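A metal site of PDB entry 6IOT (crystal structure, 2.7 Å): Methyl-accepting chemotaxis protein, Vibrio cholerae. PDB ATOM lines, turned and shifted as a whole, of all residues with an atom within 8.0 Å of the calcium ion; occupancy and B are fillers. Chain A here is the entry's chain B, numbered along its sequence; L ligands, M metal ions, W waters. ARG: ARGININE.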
ATOM      1  N   LYS A  58     -11.109   0.768   5.218  1.00  0.00           N
ATOM      2  CA  LYS A  58     -10.935  -0.659   4.975  1.00  0.00           C
ATOM      3  C   LYS A  58     -12.012  -1.473   5.679  1.00  0.00           C
ATOM      4  O   LYS A  58     -12.604  -2.367   5.089  1.00  0.00           O
ATOM      5  CB  LYS A  58      -9.550  -1.119   5.438  1.00  0.00           C
ATOM      6  CG  LYS A  58      -9.273  -2.598   5.193  1.00  0.00           C
ATOM      7  CD  LYS A  58      -7.937  -3.026   5.772  1.00  0.00           C
ATOM      8  CE  LYS A  58      -7.616  -4.467   5.421  1.00  0.00           C
ATOM      9  NZ  LYS A  58      -7.364  -4.645   3.967  1.00  0.00           N
ATOM     10  N   GLU A  62     -14.652  -3.903   3.768  1.00  0.00           N
ATOM     11  CA  GLU A  62     -14.500  -5.332   4.016  1.00  0.00           C
ATOM     12  C   GLU A  62     -15.747  -5.954   4.640  1.00  0.00           C
ATOM     13  O   GLU A  62     -15.782  -7.154   4.895  1.00  0.00           O
ATOM     14  CB  GLU A  62     -13.295  -5.599   4.920  1.00  0.00           C
ATOM     15  CG  GLU A  62     -11.946  -5.239   4.311  1.00  0.00           C
ATOM     16  CD  GLU A  62     -11.523  -6.168   3.194  1.00  0.00           C
ATOM     17  OE1 GLU A  62     -12.171  -7.216   3.002  1.00  0.00           O
ATOM     18  OE2 GLU A  62     -10.535  -5.846   2.495  1.00  0.00           O
ATOM     19  N   LYS A  67     -18.866  -6.023   0.451  1.00  0.00           N
ATOM     20  CA  LYS A  67     -17.806  -6.749  -0.249  1.00  0.00           C
ATOM     21  C   LYS A  67     -18.368  -7.746  -1.255  1.00  0.00           C
ATOM     22  O   LYS A  67     -17.744  -8.033  -2.281  1.00  0.00           O
ATOM     23  CB  LYS A  67     -16.905  -7.468   0.745  1.00  0.00           C
ATOM     24  CG  LYS A  67     -15.595  -7.991   0.171  1.00  0.00           C
ATOM     25  CD  LYS A  67     -14.960  -9.015   1.096  1.00  0.00           C
ATOM     26  CE  LYS A  67     -13.467  -9.147   0.840  1.00  0.00           C
ATOM     27  NZ  LYS A  67     -13.141  -9.346  -0.597  1.00  0.00           N
ATOM     28  N   ALA A  72     -15.122  -5.375  -6.757  1.00  0.00           N
ATOM     29  CA  ALA A  72     -14.122  -4.776  -5.880  1.00  0.00           C
ATOM     30  C   ALA A  72     -14.481  -3.326  -5.606  1.00  0.00           C
ATOM     31  O   ALA A  72     -15.120  -2.670  -6.416  1.00  0.00           O
ATOM     32  CB  ALA A  72     -12.746  -4.883  -6.502  1.00  0.00           C
ATOM     33  N   ILE A  73     -14.060  -2.832  -4.439  1.00  0.00           N
ATOM     34  CA  ILE A  73     -14.294  -1.442  -4.072  1.00  0.00           C
ATOM     35  C   ILE A  73     -13.002  -0.812  -3.573  1.00  0.00           C
ATOM     36  O   ILE A  73     -12.279  -1.423  -2.792  1.00  0.00           O
ATOM     37  CB  ILE A  73     -15.390  -1.301  -2.992  1.00  0.00           C
ATOM     38  CG1 ILE A  73     -16.638  -2.081  -3.392  1.00  0.00           C
ATOM     39  CG2 ILE A  73     -15.720   0.161  -2.763  1.00  0.00           C
ATOM     40  CD1 ILE A  73     -17.564  -2.360  -2.231  1.00  0.00           C
ATOM     41  N   VAL A  83      -4.122   3.985  -2.647  1.00  0.00           N
ATOM     42  CA  VAL A  83      -5.415   3.328  -2.825  1.00  0.00           C
ATOM     43  C   VAL A  83      -5.745   2.328  -1.716  1.00  0.00           C
ATOM     44  O   VAL A  83      -4.987   1.379  -1.499  1.00  0.00           O
ATOM     45  CB  VAL A  83      -5.494   2.595  -4.177  1.00  0.00           C
ATOM     46  CG1 VAL A  83      -6.915   2.133  -4.442  1.00  0.00           C
ATOM     47  CG2 VAL A  83      -5.008   3.482  -5.312  1.00  0.00           C
ATOM     48  N   VAL A  84      -6.864   2.533  -1.045  1.00  0.00           N
ATOM     49  CA  VAL A  84      -7.418   1.546  -0.132  1.00  0.00           C
ATOM     50  C   VAL A  84      -8.509   0.755  -0.860  1.00  0.00           C
ATOM     51  O   VAL A  84      -9.509   1.335  -1.282  1.00  0.00           O
ATOM     52  CB  VAL A  84      -8.014   2.192   1.139  1.00  0.00           C
ATOM     53  CG1 VAL A  84      -8.571   1.112   2.061  1.00  0.00           C
ATOM     54  CG2 VAL A  84      -6.967   3.036   1.843  1.00  0.00           C
ATOM     55  N   GLU A  85      -8.323  -0.545  -1.023  1.00  0.00           N
ATOM     56  CA  GLU A  85      -9.296  -1.368  -1.736  1.00  0.00           C
ATOM     57  C   GLU A  85      -9.497  -2.724  -1.070  1.00  0.00           C
ATOM     58  O   GLU A  85      -8.707  -3.131  -0.218  1.00  0.00           O
ATOM     59  CB  GLU A  85      -8.862  -1.554  -3.192  1.00  0.00           C
ATOM     60  CG  GLU A  85      -8.234  -2.905  -3.536  1.00  0.00           C
ATOM     61  CD  GLU A  85      -6.780  -2.995  -3.145  1.00  0.00           C
ATOM     62  OE1 GLU A  85      -6.304  -2.136  -2.380  1.00  0.00           O
ATOM     63  OE2 GLU A  85      -6.097  -3.924  -3.624  1.00  0.00           O
ATOM     64  N   ASN A  86     -10.567  -3.424  -1.461  1.00  0.00           N
ATOM     65  CA  ASN A  86     -10.983  -4.643  -0.769  1.00  0.00           C
ATOM     66  C   ASN A  86     -10.808  -5.934  -1.563  1.00  0.00           C
ATOM     67  O   ASN A  86     -11.414  -6.953  -1.224  1.00  0.00           O
ATOM     68  CB  ASN A  86     -12.451  -4.508  -0.338  1.00  0.00           C
ATOM     69  CG  ASN A  86     -13.388  -4.378  -1.518  1.00  0.00           C
ATOM     70  OD1 ASN A  86     -12.962  -4.223  -2.665  1.00  0.00           O
ATOM     71  ND2 ASN A  86     -14.691  -4.423  -1.251  1.00  0.00           N
ATOM     72  N   ASP A  87     -10.003  -5.901  -2.618  1.00  0.00           N
ATOM     73  CA  ASP A  87      -9.765  -7.093  -3.425  1.00  0.00           C
ATOM     74  C   ASP A  87      -8.616  -7.909  -2.837  1.00  0.00           C
ATOM     75  O   ASP A  87      -7.449  -7.534  -2.956  1.00  0.00           O
ATOM     76  CB  ASP A  87      -9.472  -6.729  -4.881  1.00  0.00           C
ATOM     77  CG  ASP A  87      -9.537  -7.928  -5.811  1.00  0.00           C
ATOM     78  OD1 ASP A  87      -9.708  -9.060  -5.322  1.00  0.00           O
ATOM     79  OD2 ASP A  87      -9.415  -7.730  -7.035  1.00  0.00           O
ATOM     80  N   ASP A  88      -8.937  -9.046  -2.227  1.00  0.00           N
ATOM     81  CA  ASP A  88      -7.941  -9.891  -1.576  1.00  0.00           C
ATOM     82  C   ASP A  88      -6.901 -10.428  -2.548  1.00  0.00           C
ATOM     83  O   ASP A  88      -5.797 -10.803  -2.137  1.00  0.00           O
ATOM     84  CB  ASP A  88      -8.629 -11.049  -0.849  1.00  0.00           C
ATOM     85  CG  ASP A  88      -9.611 -10.587   0.206  1.00  0.00           C
ATOM     86  OD1 ASP A  88      -9.486  -9.433   0.671  1.00  0.00           O
ATOM     87  OD2 ASP A  88     -10.502 -11.380   0.573  1.00  0.00           O
ATOM     88  N   GLY A  89      -7.238 -10.465  -3.822  1.00  0.00           N
ATOM     89  CA  GLY A  89      -6.329 -10.974  -4.841  1.00  0.00           C
ATOM     90  C   GLY A  89      -5.603  -9.882  -5.595  1.00  0.00           C
ATOM     91  O   GLY A  89      -4.880 -10.154  -6.549  1.00  0.00           O
ATOM     92  N   TRP A  90      -5.787  -8.640  -5.170  1.00  0.00           N
ATOM     93  CA  TRP A  90      -5.184  -7.515  -5.876  1.00  0.00           C
ATOM     94  C   TRP A  90      -4.448  -6.530  -4.967  1.00  0.00           C
ATOM     95  O   TRP A  90      -4.813  -6.331  -3.814  1.00  0.00           O
ATOM     96  CB  TRP A  90      -6.243  -6.757  -6.683  1.00  0.00           C
ATOM     97  CG  TRP A  90      -5.669  -5.719  -7.612  1.00  0.00           C
ATOM     98  CD1 TRP A  90      -4.782  -5.935  -8.625  1.00  0.00           C
ATOM     99  CD2 TRP A  90      -5.939  -4.319  -7.600  1.00  0.00           C
ATOM    100  NE1 TRP A  90      -4.488  -4.742  -9.258  1.00  0.00           N
ATOM    101  CE2 TRP A  90      -5.193  -3.733  -8.642  1.00  0.00           C
ATOM    102  CE3 TRP A  90      -6.753  -3.490  -6.823  1.00  0.00           C
ATOM    103  CZ2 TRP A  90      -5.217  -2.374  -8.917  1.00  0.00           C
ATOM    104  CZ3 TRP A  90      -6.783  -2.136  -7.093  1.00  0.00           C
ATOM    105  CH2 TRP A  90      -6.016  -1.587  -8.134  1.00  0.00           C
ATOM    106  N   GLU A  91      -3.403  -5.932  -5.521  1.00  0.00           N
ATOM    107  CA  GLU A  91      -2.699  -4.794  -4.945  1.00  0.00           C
ATOM    108  C   GLU A  91      -2.184  -3.954  -6.115  1.00  0.00           C
ATOM    109  O   GLU A  91      -1.461  -4.472  -6.967  1.00  0.00           O
ATOM    110  CB  GLU A  91      -1.546  -5.224  -4.043  1.00  0.00           C
ATOM    111  CG  GLU A  91      -0.984  -4.108  -3.173  1.00  0.00           C
ATOM    112  CD  GLU A  91      -1.936  -3.682  -2.058  1.00  0.00           C
ATOM    113  OE1 GLU A  91      -2.184  -4.508  -1.157  1.00  0.00           O
ATOM    114  OE2 GLU A  91      -2.434  -2.541  -2.085  1.00  0.00           O
ATOM    115  N   PRO A  92      -2.552  -2.668  -6.151  1.00  0.00           N
ATOM    116  CA  PRO A  92      -2.115  -1.802  -7.252  1.00  0.00           C
ATOM    117  C   PRO A  92      -0.593  -1.737  -7.379  1.00  0.00           C
ATOM    118  O   PRO A  92       0.080  -1.389  -6.412  1.00  0.00           O
ATOM    119  CB  PRO A  92      -2.696  -0.440  -6.885  1.00  0.00           C
ATOM    120  CG  PRO A  92      -2.925  -0.504  -5.405  1.00  0.00           C
ATOM    121  CD  PRO A  92      -3.306  -1.925  -5.134  1.00  0.00           C
HETATM  122  N   ARG L   1     -11.960  -0.388 -11.155  1.00  0.00           N
HETATM  123  CA  ARG L   1     -10.506  -0.442 -11.127  1.00  0.00           C
HETATM  124  C   ARG L   1      -9.915  -0.202 -12.502  1.00  0.00           C
HETATM  125  O   ARG L   1      -9.035   0.644 -12.682  1.00  0.00           O
HETATM  126  CB  ARG L   1     -10.035  -1.796 -10.578  1.00  0.00           C
HETATM  127  CG  ARG L   1      -8.539  -2.035 -10.732  1.00  0.00           C
HETATM  128  CD  ARG L   1      -8.203  -3.517 -10.661  1.00  0.00           C
HETATM  129  NE  ARG L   1      -8.597  -4.120  -9.390  1.00  0.00           N
HETATM  130  CZ  ARG L   1      -9.641  -4.912  -9.232  1.00  0.00           C
HETATM  131  NH1 ARG L   1      -9.920  -5.423  -8.032  1.00  0.00           N
HETATM  132  NH2 ARG L   1     -10.416  -5.216 -10.268  1.00  0.00           N
HETATM  133  OXT ARG L   1     -10.301  -0.847 -13.479  1.00  0.00           O
HETATM  134 CA    CA M   1      -6.741  -5.562  -1.964  1.00  0.00          CA
HETATM  135  O   HOH W   1      -5.010  -7.742  -1.906  1.00  0.00           O
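OD2 of Asp 87 lies within salt-bridge range of NH1 of the ligand, 2.6 Å away.
The backbone NH (N) of Gly 89 lies close to the side-chain carboxylate (OD1) of Asp 87, at 3.2 Å.
The calcium ion is bound by O of Asp 87 (2.3 Å), OE2 of Glu 85 (2.4 Å), O of Trp 90 (2.8 Å) and water W1 (2.8 Å).
The calcium ion has four donor atoms within binding distance.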
